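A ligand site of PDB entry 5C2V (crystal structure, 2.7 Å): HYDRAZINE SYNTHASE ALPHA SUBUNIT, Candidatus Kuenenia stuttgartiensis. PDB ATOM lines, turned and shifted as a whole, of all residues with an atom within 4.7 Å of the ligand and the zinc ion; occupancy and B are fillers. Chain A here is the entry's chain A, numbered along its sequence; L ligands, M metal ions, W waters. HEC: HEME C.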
ATOM      1  N   ARG A 250     -19.954 -40.024 -10.485  1.00  0.00           N
ATOM      2  CA  ARG A 250     -18.563 -39.579 -10.547  1.00  0.00           C
ATOM      3  C   ARG A 250     -17.585 -40.562  -9.915  1.00  0.00           C
ATOM      4  O   ARG A 250     -17.977 -41.374  -9.066  1.00  0.00           O
ATOM      5  CB  ARG A 250     -18.407 -38.212  -9.864  1.00  0.00           C
ATOM      6  CG  ARG A 250     -18.403 -38.282  -8.338  1.00  0.00           C
ATOM      7  CD  ARG A 250     -18.101 -36.928  -7.720  1.00  0.00           C
ATOM      8  NE  ARG A 250     -16.832 -36.387  -8.194  1.00  0.00           N
ATOM      9  CZ  ARG A 250     -15.664 -36.567  -7.581  1.00  0.00           C
ATOM     10  NH1 ARG A 250     -15.613 -37.274  -6.464  1.00  0.00           N
ATOM     11  NH2 ARG A 250     -14.562 -36.036  -8.086  1.00  0.00           N
ATOM     12  N   MET A 258     -11.991 -36.799   0.061  1.00  0.00           N
ATOM     13  CA  MET A 258     -10.905 -35.856  -0.183  1.00  0.00           C
ATOM     14  C   MET A 258     -10.521 -35.071   1.060  1.00  0.00           C
ATOM     15  O   MET A 258     -11.363 -34.792   1.924  1.00  0.00           O
ATOM     16  CB  MET A 258     -11.289 -34.890  -1.297  1.00  0.00           C
ATOM     17  CG  MET A 258     -12.341 -33.853  -0.906  1.00  0.00           C
ATOM     18  SD  MET A 258     -12.469 -32.493  -2.079  1.00  0.00           S
ATOM     19  CE  MET A 258     -13.789 -31.530  -1.334  1.00  0.00           C
ATOM     20  N   PRO A 269     -14.772 -23.017   0.473  1.00  0.00           N
ATOM     21  CA  PRO A 269     -14.290 -24.394   0.395  1.00  0.00           C
ATOM     22  C   PRO A 269     -13.397 -24.645  -0.819  1.00  0.00           C
ATOM     23  O   PRO A 269     -13.743 -24.229  -1.933  1.00  0.00           O
ATOM     24  CB  PRO A 269     -15.581 -25.213   0.297  1.00  0.00           C
ATOM     25  CG  PRO A 269     -16.566 -24.285  -0.319  1.00  0.00           C
ATOM     26  CD  PRO A 269     -16.218 -22.924   0.207  1.00  0.00           C
ATOM     27  N   PRO A 271     -10.400 -27.735  -2.539  1.00  0.00           N
ATOM     28  CA  PRO A 271      -9.740 -29.038  -2.422  1.00  0.00           C
ATOM     29  C   PRO A 271      -8.251 -28.926  -2.085  1.00  0.00           C
ATOM     30  O   PRO A 271      -7.570 -28.021  -2.574  1.00  0.00           O
ATOM     31  CB  PRO A 271      -9.927 -29.641  -3.823  1.00  0.00           C
ATOM     32  CG  PRO A 271     -10.007 -28.458  -4.717  1.00  0.00           C
ATOM     33  CD  PRO A 271     -10.754 -27.413  -3.928  1.00  0.00           C
ATOM     34  N   ASN A 275      -9.321 -35.615  -4.474  1.00  0.00           N
ATOM     35  CA  ASN A 275     -10.574 -35.647  -5.227  1.00  0.00           C
ATOM     36  C   ASN A 275     -10.426 -35.691  -6.750  1.00  0.00           C
ATOM     37  O   ASN A 275     -11.393 -35.972  -7.461  1.00  0.00           O
ATOM     38  CB  ASN A 275     -11.424 -34.425  -4.861  1.00  0.00           C
ATOM     39  CG  ASN A 275     -12.857 -34.540  -5.346  1.00  0.00           C
ATOM     40  OD1 ASN A 275     -13.474 -35.600  -5.233  1.00  0.00           O
ATOM     41  ND2 ASN A 275     -13.376 -33.455  -5.916  1.00  0.00           N
ATOM     42  N   CYS A 276      -9.217 -35.447  -7.249  1.00  0.00           N
ATOM     43  CA  CYS A 276      -9.029 -35.247  -8.686  1.00  0.00           C
ATOM     44  C   CYS A 276      -8.364 -36.434  -9.373  1.00  0.00           C
ATOM     45  O   CYS A 276      -7.554 -37.141  -8.765  1.00  0.00           O
ATOM     46  CB  CYS A 276      -8.213 -33.974  -8.945  1.00  0.00           C
ATOM     47  SG  CYS A 276      -9.006 -32.443  -8.358  1.00  0.00           S
ATOM     48  N   TRP A 431     -22.413 -15.967  -7.660  1.00  0.00           N
ATOM     49  CA  TRP A 431     -21.138 -16.534  -8.100  1.00  0.00           C
ATOM     50  C   TRP A 431     -20.806 -16.140  -9.535  1.00  0.00           C
ATOM     51  O   TRP A 431     -21.700 -15.866 -10.347  1.00  0.00           O
ATOM     52  CB  TRP A 431     -21.114 -18.060  -7.938  1.00  0.00           C
ATOM     53  CG  TRP A 431     -22.096 -18.824  -8.782  1.00  0.00           C
ATOM     54  CD1 TRP A 431     -23.315 -19.287  -8.401  1.00  0.00           C
ATOM     55  CD2 TRP A 431     -21.921 -19.233 -10.149  1.00  0.00           C
ATOM     56  NE1 TRP A 431     -23.922 -19.957  -9.441  1.00  0.00           N
ATOM     57  CE2 TRP A 431     -23.086 -19.943 -10.526  1.00  0.00           C
ATOM     58  CE3 TRP A 431     -20.891 -19.074 -11.085  1.00  0.00           C
ATOM     59  CZ2 TRP A 431     -23.249 -20.475 -11.796  1.00  0.00           C
ATOM     60  CZ3 TRP A 431     -21.060 -19.611 -12.351  1.00  0.00           C
ATOM     61  CH2 TRP A 431     -22.224 -20.309 -12.692  1.00  0.00           C
ATOM     62  N   ILE A 432     -19.507 -16.108  -9.833  1.00  0.00           N
ATOM     63  CA  ILE A 432     -19.019 -15.686 -11.132  1.00  0.00           C
ATOM     64  C   ILE A 432     -17.837 -16.524 -11.621  1.00  0.00           C
ATOM     65  O   ILE A 432     -16.867 -16.782 -10.886  1.00  0.00           O
ATOM     66  CB  ILE A 432     -18.615 -14.186 -11.103  1.00  0.00           C
ATOM     67  CG1 ILE A 432     -17.995 -13.762 -12.432  1.00  0.00           C
ATOM     68  CG2 ILE A 432     -17.676 -13.897  -9.947  1.00  0.00           C
ATOM     69  CD1 ILE A 432     -17.636 -12.286 -12.493  1.00  0.00           C
ATOM     70  N   CYS A 433     -17.938 -16.965 -12.871  1.00  0.00           N
ATOM     71  CA  CYS A 433     -16.860 -17.673 -13.542  1.00  0.00           C
ATOM     72  C   CYS A 433     -16.343 -16.813 -14.694  1.00  0.00           C
ATOM     73  O   CYS A 433     -17.126 -16.363 -15.531  1.00  0.00           O
ATOM     74  CB  CYS A 433     -17.326 -19.035 -14.059  1.00  0.00           C
ATOM     75  SG  CYS A 433     -16.046 -20.000 -14.886  1.00  0.00           S
ATOM     76  N   THR A 436     -15.922 -19.927 -18.806  1.00  0.00           N
ATOM     77  CA  THR A 436     -16.582 -21.224 -18.631  1.00  0.00           C
ATOM     78  C   THR A 436     -16.023 -22.258 -19.606  1.00  0.00           C
ATOM     79  O   THR A 436     -16.223 -23.455 -19.430  1.00  0.00           O
ATOM     80  CB  THR A 436     -18.105 -21.125 -18.819  1.00  0.00           C
ATOM     81  OG1 THR A 436     -18.405 -20.346 -19.983  1.00  0.00           O
ATOM     82  CG2 THR A 436     -18.754 -20.470 -17.608  1.00  0.00           C
ATOM     83  N   GLN A 441      -9.731 -30.318 -18.308  1.00  0.00           N
ATOM     84  CA  GLN A 441     -10.295 -31.596 -18.697  1.00  0.00           C
ATOM     85  C   GLN A 441     -10.294 -31.795 -20.207  1.00  0.00           C
ATOM     86  O   GLN A 441     -10.512 -30.840 -20.962  1.00  0.00           O
ATOM     87  CB  GLN A 441     -11.718 -31.735 -18.157  1.00  0.00           C
ATOM     88  CG  GLN A 441     -11.795 -31.907 -16.650  1.00  0.00           C
ATOM     89  CD  GLN A 441     -11.057 -33.135 -16.174  1.00  0.00           C
ATOM     90  OE1 GLN A 441     -11.155 -34.203 -16.770  1.00  0.00           O
ATOM     91  NE2 GLN A 441     -10.301 -32.989 -15.089  1.00  0.00           N
ATOM     92  N   HIS A 448     -17.964 -35.514 -16.370  1.00  0.00           N
ATOM     93  CA  HIS A 448     -17.159 -34.411 -15.848  1.00  0.00           C
ATOM     94  C   HIS A 448     -16.183 -33.899 -16.910  1.00  0.00           C
ATOM     95  O   HIS A 448     -15.443 -32.937 -16.673  1.00  0.00           O
ATOM     96  CB  HIS A 448     -16.396 -34.851 -14.596  1.00  0.00           C
ATOM     97  CG  HIS A 448     -15.371 -35.914 -14.848  1.00  0.00           C
ATOM     98  ND1 HIS A 448     -15.650 -37.256 -14.693  1.00  0.00           N
ATOM     99  CD2 HIS A 448     -14.083 -35.834 -15.235  1.00  0.00           C
ATOM    100  CE1 HIS A 448     -14.567 -37.956 -14.978  1.00  0.00           C
ATOM    101  NE2 HIS A 448     -13.599 -37.122 -15.301  1.00  0.00           N
ATOM    102  N   MET A 529     -23.397 -26.864 -11.328  1.00  0.00           N
ATOM    103  CA  MET A 529     -23.716 -26.242 -12.602  1.00  0.00           C
ATOM    104  C   MET A 529     -23.310 -27.083 -13.808  1.00  0.00           C
ATOM    105  O   MET A 529     -22.529 -28.027 -13.696  1.00  0.00           O
ATOM    106  CB  MET A 529     -23.048 -24.868 -12.684  1.00  0.00           C
ATOM    107  CG  MET A 529     -21.533 -24.929 -12.550  1.00  0.00           C
ATOM    108  SD  MET A 529     -20.890 -23.640 -11.475  1.00  0.00           S
ATOM    109  CE  MET A 529     -21.618 -24.126  -9.915  1.00  0.00           C
ATOM    110  N   GLN A 530     -23.861 -26.715 -14.964  1.00  0.00           N
ATOM    111  CA  GLN A 530     -23.504 -27.335 -16.241  1.00  0.00           C
ATOM    112  C   GLN A 530     -23.415 -26.261 -17.326  1.00  0.00           C
ATOM    113  O   GLN A 530     -24.301 -25.416 -17.429  1.00  0.00           O
ATOM    114  CB  GLN A 530     -24.522 -28.396 -16.641  1.00  0.00           C
ATOM    115  CG  GLN A 530     -24.542 -29.632 -15.764  1.00  0.00           C
ATOM    116  CD  GLN A 530     -25.682 -30.571 -16.114  1.00  0.00           C
ATOM    117  OE1 GLN A 530     -26.745 -30.134 -16.552  1.00  0.00           O
ATOM    118  NE2 GLN A 530     -25.453 -31.864 -15.944  1.00  0.00           N
ATOM    119  N   ILE A 531     -22.354 -26.295 -18.129  1.00  0.00           N
ATOM    120  CA  ILE A 531     -22.223 -25.357 -19.234  1.00  0.00           C
ATOM    121  C   ILE A 531     -23.003 -25.865 -20.443  1.00  0.00           C
ATOM    122  O   ILE A 531     -23.008 -27.066 -20.729  1.00  0.00           O
ATOM    123  CB  ILE A 531     -20.755 -25.103 -19.608  1.00  0.00           C
ATOM    124  CG1 ILE A 531     -20.038 -26.413 -19.932  1.00  0.00           C
ATOM    125  CG2 ILE A 531     -20.037 -24.373 -18.486  1.00  0.00           C
ATOM    126  CD1 ILE A 531     -18.586 -26.231 -20.321  1.00  0.00           C
ATOM    127  N   GLN A 540     -20.372 -30.062 -20.317  1.00  0.00           N
ATOM    128  CA  GLN A 540     -19.550 -30.519 -19.204  1.00  0.00           C
ATOM    129  C   GLN A 540     -20.297 -30.295 -17.884  1.00  0.00           C
ATOM    130  O   GLN A 540     -20.976 -29.284 -17.713  1.00  0.00           O
ATOM    131  CB  GLN A 540     -18.216 -29.789 -19.197  1.00  0.00           C
ATOM    132  CG  GLN A 540     -17.201 -30.321 -18.207  1.00  0.00           C
ATOM    133  CD  GLN A 540     -15.854 -29.628 -18.343  1.00  0.00           C
ATOM    134  OE1 GLN A 540     -15.654 -28.808 -19.242  1.00  0.00           O
ATOM    135  NE2 GLN A 540     -14.926 -29.957 -17.458  1.00  0.00           N
ATOM    136  N   THR A 541     -20.171 -31.244 -16.969  1.00  0.00           N
ATOM    137  CA  THR A 541     -20.861 -31.163 -15.692  1.00  0.00           C
ATOM    138  C   THR A 541     -19.864 -31.018 -14.541  1.00  0.00           C
ATOM    139  O   THR A 541     -18.855 -31.715 -14.496  1.00  0.00           O
ATOM    140  CB  THR A 541     -21.740 -32.401 -15.450  1.00  0.00           C
ATOM    141  OG1 THR A 541     -22.626 -32.579 -16.555  1.00  0.00           O
ATOM    142  CG2 THR A 541     -22.561 -32.245 -14.166  1.00  0.00           C
ATOM    143  N   ALA A 542     -20.157 -30.123 -13.607  1.00  0.00           N
ATOM    144  CA  ALA A 542     -19.368 -30.026 -12.400  1.00  0.00           C
ATOM    145  C   ALA A 542     -20.002 -30.917 -11.349  1.00  0.00           C
ATOM    146  O   ALA A 542     -21.071 -30.613 -10.838  1.00  0.00           O
ATOM    147  CB  ALA A 542     -19.281 -28.590 -11.911  1.00  0.00           C
ATOM    148  N   LEU A 543     -19.345 -32.024 -11.033  1.00  0.00           N
ATOM    149  CA  LEU A 543     -19.924 -32.979 -10.093  1.00  0.00           C
ATOM    150  C   LEU A 543     -19.287 -32.798  -8.732  1.00  0.00           C
ATOM    151  O   LEU A 543     -18.148 -33.212  -8.491  1.00  0.00           O
ATOM    152  CB  LEU A 543     -19.738 -34.407 -10.601  1.00  0.00           C
ATOM    153  CG  LEU A 543     -20.536 -34.765 -11.867  1.00  0.00           C
ATOM    154  CD1 LEU A 543     -20.087 -36.112 -12.420  1.00  0.00           C
ATOM    155  CD2 LEU A 543     -22.031 -34.778 -11.592  1.00  0.00           C
ATOM    156  N   THR A 544     -20.070 -32.200  -7.842  1.00  0.00           N
ATOM    157  CA  THR A 544     -19.638 -31.780  -6.516  1.00  0.00           C
ATOM    158  C   THR A 544     -20.810 -31.018  -5.927  1.00  0.00           C
ATOM    159  O   THR A 544     -21.770 -30.708  -6.632  1.00  0.00           O
ATOM    160  CB  THR A 544     -18.400 -30.872  -6.550  1.00  0.00           C
ATOM    161  OG1 THR A 544     -17.962 -30.605  -5.208  1.00  0.00           O
ATOM    162  CG2 THR A 544     -18.719 -29.565  -7.253  1.00  0.00           C
ATOM    163  N   ARG A 554     -18.878 -15.901  -4.920  1.00  0.00           N
ATOM    164  CA  ARG A 554     -17.804 -16.865  -5.119  1.00  0.00           C
ATOM    165  C   ARG A 554     -17.227 -16.779  -6.534  1.00  0.00           C
ATOM    166  O   ARG A 554     -17.966 -16.862  -7.508  1.00  0.00           O
ATOM    167  CB  ARG A 554     -18.289 -18.298  -4.848  1.00  0.00           C
ATOM    168  CG  ARG A 554     -17.215 -19.364  -4.988  1.00  0.00           C
ATOM    169  CD  ARG A 554     -16.083 -19.162  -3.991  1.00  0.00           C
ATOM    170  NE  ARG A 554     -14.945 -20.031  -4.244  1.00  0.00           N
ATOM    171  CZ  ARG A 554     -14.721 -21.190  -3.631  1.00  0.00           C
ATOM    172  NH1 ARG A 554     -15.583 -21.631  -2.719  1.00  0.00           N
ATOM    173  NH2 ARG A 554     -13.655 -21.912  -3.941  1.00  0.00           N
ATOM    174  N   ILE A 555     -15.916 -16.613  -6.632  1.00  0.00           N
ATOM    175  CA  ILE A 555     -15.270 -16.440  -7.935  1.00  0.00           C
ATOM    176  C   ILE A 555     -14.488 -17.684  -8.363  1.00  0.00           C
ATOM    177  O   ILE A 555     -13.983 -18.429  -7.523  1.00  0.00           O
ATOM    178  CB  ILE A 555     -14.309 -15.232  -7.942  1.00  0.00           C
ATOM    179  CG1 ILE A 555     -13.070 -15.519  -7.089  1.00  0.00           C
ATOM    180  CG2 ILE A 555     -15.025 -13.979  -7.450  1.00  0.00           C
ATOM    181  CD1 ILE A 555     -11.996 -14.453  -7.201  1.00  0.00           C
ATOM    182  N   CYS A 556     -14.422 -17.913  -9.663  1.00  0.00           N
ATOM    183  CA  CYS A 556     -13.523 -18.935 -10.204  1.00  0.00           C
ATOM    184  C   CYS A 556     -13.034 -18.549 -11.601  1.00  0.00           C
ATOM    185  O   CYS A 556     -13.790 -17.997 -12.394  1.00  0.00           O
ATOM    186  CB  CYS A 556     -14.199 -20.300 -10.226  1.00  0.00           C
ATOM    187  SG  CYS A 556     -15.747 -20.349 -11.165  1.00  0.00           S
ATOM    188  N   GLY A 558     -12.116 -20.541 -14.116  1.00  0.00           N
ATOM    189  CA  GLY A 558     -12.502 -21.419 -15.190  1.00  0.00           C
ATOM    190  C   GLY A 558     -13.322 -22.607 -14.745  1.00  0.00           C
ATOM    191  O   GLY A 558     -13.764 -22.679 -13.593  1.00  0.00           O
ATOM    192  N   CYS A 559     -13.520 -23.548 -15.647  1.00  0.00           N
ATOM    193  CA  CYS A 559     -14.289 -24.736 -15.334  1.00  0.00           C
ATOM    194  C   CYS A 559     -13.297 -25.851 -15.006  1.00  0.00           C
ATOM    195  O   CYS A 559     -12.715 -26.454 -15.891  1.00  0.00           O
ATOM    196  CB  CYS A 559     -15.180 -25.107 -16.524  1.00  0.00           C
ATOM    197  SG  CYS A 559     -16.204 -26.580 -16.370  1.00  0.00           S
ATOM    198  N   HIS A 560     -13.174 -26.134 -13.711  1.00  0.00           N
ATOM    199  CA  HIS A 560     -12.115 -27.004 -13.194  1.00  0.00           C
ATOM    200  C   HIS A 560     -10.746 -26.697 -13.826  1.00  0.00           C
ATOM    201  O   HIS A 560     -10.054 -27.603 -14.283  1.00  0.00           O
ATOM    202  CB  HIS A 560     -12.473 -28.480 -13.400  1.00  0.00           C
ATOM    203  CG  HIS A 560     -11.697 -29.412 -12.519  1.00  0.00           C
ATOM    204  ND1 HIS A 560     -10.510 -29.999 -12.922  1.00  0.00           N
ATOM    205  CD2 HIS A 560     -11.934 -29.852 -11.260  1.00  0.00           C
ATOM    206  CE1 HIS A 560     -10.055 -30.766 -11.951  1.00  0.00           C
ATOM    207  NE2 HIS A 560     -10.893 -30.692 -10.923  1.00  0.00           N
ATOM    208  N   TYR A 564      -8.981 -23.020  -8.186  1.00  0.00           N
ATOM    209  CA  TYR A 564      -9.229 -23.471  -6.809  1.00  0.00           C
ATOM    210  C   TYR A 564      -8.461 -24.733  -6.427  1.00  0.00           C
ATOM    211  O   TYR A 564      -8.655 -25.240  -5.319  1.00  0.00           O
ATOM    212  CB  TYR A 564     -10.739 -23.658  -6.551  1.00  0.00           C
ATOM    213  CG  TYR A 564     -11.554 -24.312  -7.654  1.00  0.00           C
ATOM    214  CD1 TYR A 564     -11.710 -25.688  -7.705  1.00  0.00           C
ATOM    215  CD2 TYR A 564     -12.221 -23.537  -8.600  1.00  0.00           C
ATOM    216  CE1 TYR A 564     -12.484 -26.278  -8.701  1.00  0.00           C
ATOM    217  CE2 TYR A 564     -12.982 -24.123  -9.593  1.00  0.00           C
ATOM    218  CZ  TYR A 564     -13.120 -25.494  -9.633  1.00  0.00           C
ATOM    219  OH  TYR A 564     -13.892 -26.076 -10.618  1.00  0.00           O
ATOM    220  N   ARG A 565      -7.608 -25.257  -7.303  1.00  0.00           N
ATOM    221  CA  ARG A 565      -6.854 -26.452  -6.934  1.00  0.00           C
ATOM    222  C   ARG A 565      -5.326 -26.279  -6.890  1.00  0.00           C
ATOM    223  O   ARG A 565      -4.759 -26.056  -5.818  1.00  0.00           O
ATOM    224  CB  ARG A 565      -7.212 -27.591  -7.886  1.00  0.00           C
ATOM    225  CG  ARG A 565      -6.449 -28.898  -7.683  1.00  0.00           C
ATOM    226  CD  ARG A 565      -6.683 -29.500  -6.319  1.00  0.00           C
ATOM    227  NE  ARG A 565      -5.857 -30.680  -6.097  1.00  0.00           N
ATOM    228  CZ  ARG A 565      -4.639 -30.648  -5.563  1.00  0.00           C
ATOM    229  NH1 ARG A 565      -4.101 -29.491  -5.194  1.00  0.00           N
ATOM    230  NH2 ARG A 565      -3.951 -31.769  -5.401  1.00  0.00           N
HETATM  231 FE   HEC L   1     -15.830 -26.642 -10.315  1.00  0.00          FE
HETATM  232  CHA HEC L   1     -15.270 -29.833  -9.085  1.00  0.00           C
HETATM  233  CHB HEC L   1     -15.567 -25.403  -7.122  1.00  0.00           C
HETATM  234  CHC HEC L   1     -16.996 -23.571 -11.386  1.00  0.00           C
HETATM  235  CHD HEC L   1     -16.258 -27.896 -13.455  1.00  0.00           C
HETATM  236  NA  HEC L   1     -15.542 -27.470  -8.453  1.00  0.00           N
HETATM  237  C1A HEC L   1     -15.220 -28.786  -8.189  1.00  0.00           C
HETATM  238  C2A HEC L   1     -14.813 -28.894  -6.808  1.00  0.00           C
HETATM  239  C3A HEC L   1     -14.893 -27.675  -6.257  1.00  0.00           C
HETATM  240  C4A HEC L   1     -15.354 -26.753  -7.282  1.00  0.00           C
HETATM  241  CMA HEC L   1     -14.557 -27.296  -4.806  1.00  0.00           C
HETATM  242  CAA HEC L   1     -14.370 -30.200  -6.106  1.00  0.00           C
HETATM  243  CBA HEC L   1     -12.863 -30.215  -5.917  1.00  0.00           C
HETATM  244  CGA HEC L   1     -12.155 -30.401  -7.233  1.00  0.00           C
HETATM  245  O1A HEC L   1     -11.201 -29.632  -7.523  1.00  0.00           O
HETATM  246  O2A HEC L   1     -12.536 -31.326  -7.996  1.00  0.00           O
HETATM  247  NB  HEC L   1     -16.341 -24.837  -9.396  1.00  0.00           N
HETATM  248  C1B HEC L   1     -15.885 -24.503  -8.125  1.00  0.00           C
HETATM  249  C2B HEC L   1     -15.809 -23.060  -8.040  1.00  0.00           C
HETATM  250  C3B HEC L   1     -16.205 -22.554  -9.216  1.00  0.00           C
HETATM  251  C4B HEC L   1     -16.551 -23.655 -10.091  1.00  0.00           C
HETATM  252  CMB HEC L   1     -15.352 -22.244  -6.822  1.00  0.00           C
HETATM  253  CAB HEC L   1     -16.275 -21.048  -9.551  1.00  0.00           C
HETATM  254  CBB HEC L   1     -17.744 -20.624  -9.735  1.00  0.00           C
HETATM  255  NC  HEC L   1     -16.453 -25.847 -12.105  1.00  0.00           N
HETATM  256  C1C HEC L   1     -16.993 -24.597 -12.305  1.00  0.00           C
HETATM  257  C2C HEC L   1     -17.467 -24.523 -13.677  1.00  0.00           C
HETATM  258  C3C HEC L   1     -17.363 -25.739 -14.209  1.00  0.00           C
HETATM  259  C4C HEC L   1     -16.653 -26.588 -13.256  1.00  0.00           C
HETATM  260  CMC HEC L   1     -18.268 -23.350 -14.282  1.00  0.00           C
HETATM  261  CAC HEC L   1     -17.809 -26.132 -15.633  1.00  0.00           C
HETATM  262  CBC HEC L   1     -18.947 -27.167 -15.562  1.00  0.00           C
HETATM  263  ND  HEC L   1     -15.826 -28.583 -11.131  1.00  0.00           N
HETATM  264  C1D HEC L   1     -15.902 -28.819 -12.504  1.00  0.00           C
HETATM  265  C2D HEC L   1     -15.537 -30.188 -12.769  1.00  0.00           C
HETATM  266  C3D HEC L   1     -15.228 -30.794 -11.390  1.00  0.00           C
HETATM  267  C4D HEC L   1     -15.434 -29.720 -10.451  1.00  0.00           C
HETATM  268  CMD HEC L   1     -15.474 -30.888 -14.149  1.00  0.00           C
HETATM  269  CAD HEC L   1     -14.777 -32.242 -11.072  1.00  0.00           C
HETATM  270  CBD HEC L   1     -15.922 -33.217 -11.322  1.00  0.00           C
HETATM  271  CGD HEC L   1     -15.477 -34.601 -10.926  1.00  0.00           C
HETATM  272  O1D HEC L   1     -16.295 -35.551 -11.037  1.00  0.00           O
HETATM  273  O2D HEC L   1     -14.302 -34.750 -10.499  1.00  0.00           O
HETATM  274 ZN    ZN M   1     -11.059 -32.034  -9.402  1.00  0.00          ZN
HETATM  275  O   HOH W   1      -9.689 -28.415  -9.766  1.00  0.00           O
HETATM  276  O   HOH W   2     -11.746 -33.855 -10.165  1.00  0.00           O
HETATM  277  O   HOH W   3     -18.980 -25.028  -8.251  1.00  0.00           O
HETATM  278  O   HOH W   4     -15.725 -38.142 -11.879  1.00  0.00           O
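The backbone carbonyl oxygen (O) of Pro 269 lies within hydrogen-bond range of the guanidinium group (NH2) of Arg 554, at 3.1 Å.
N of Ala 542 is in hydrogen-bond range of O of Met 529, 3.2 Å away.
N of Ile 432 lies within hydrogen-bond range of O of Arg 554 (2.9 Å).
The backbone NH of Ile 531 is in hydrogen-bond range of the backbone carbonyl oxygen of Gln 540 (3.3 Å).
N of Cys 556 lies within hydrogen-bond range of O of Ile 432 (3.0 Å).
The side-chain sulfur (SG) of Cys 556 lies close to the side-chain sulfur (SG) of Cys 433 (3.7 Å).
NE of Arg 250 is in hydrogen-bond range of O of Leu 543, 3.4 Å away.
OE1 of Gln 540 sits close to SG of Cys 559, 3.7 Å away.
Water W2 lies within hydrogen-bond range of an oxygen (O2D) of the ligand and the backbone carbonyl oxygen of Asn 275.
Water W4 lies within hydrogen-bond range of O1D of the ligand (2.8 Å) and ND1 of His 448 (3.0 Å).
CAB of the ligand is covalently linked to SG of Cys 556.
SG of Cys 559 is bonded to CAC of the ligand, 1.8 Å away.
ND2 of Asn 275 sits close to O2A of the ligand, 3.1 Å away.
The guanidinium group (NH2) of Arg 250 lies within salt-bridge range of an oxygen (O2D) of the ligand (2.7 Å).
The side-chain hydroxyl (OH) of Tyr 564 binds an iron atom (FE) of the ligand.
Residues that only touch the ligand: His 448 (3.3 Å), Pro 271 (3.3 Å), Arg 554 (3.4 Å), Ala 542 (3.4 Å), Gln 540 (3.5 Å), Thr 541 (3.5 Å), Leu 543 (3.6 Å), Thr 544 (3.7 Å), Trp 431 (3.8 Å), Met 529 (3.9 Å), Gly 558 (3.97 Å) and Ile 555 (3.99 Å).
Hydrophobic or aromatic side chains that line the ligand: Pro 271, Trp 431, His 448, Met 529, Ala 542, Leu 543, His 560 and Tyr 564.
The zinc ion is bound by a ring nitrogen (NE2) of His 560 (2.0 Å), water W2 (2.1 Å), an oxygen (O2A) of the ligand (2.2 Å) and the side-chain sulfur of Cys 276 (2.3 Å).
Of the 28 residues printed, 2 come within 4 Å of the zinc ion.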
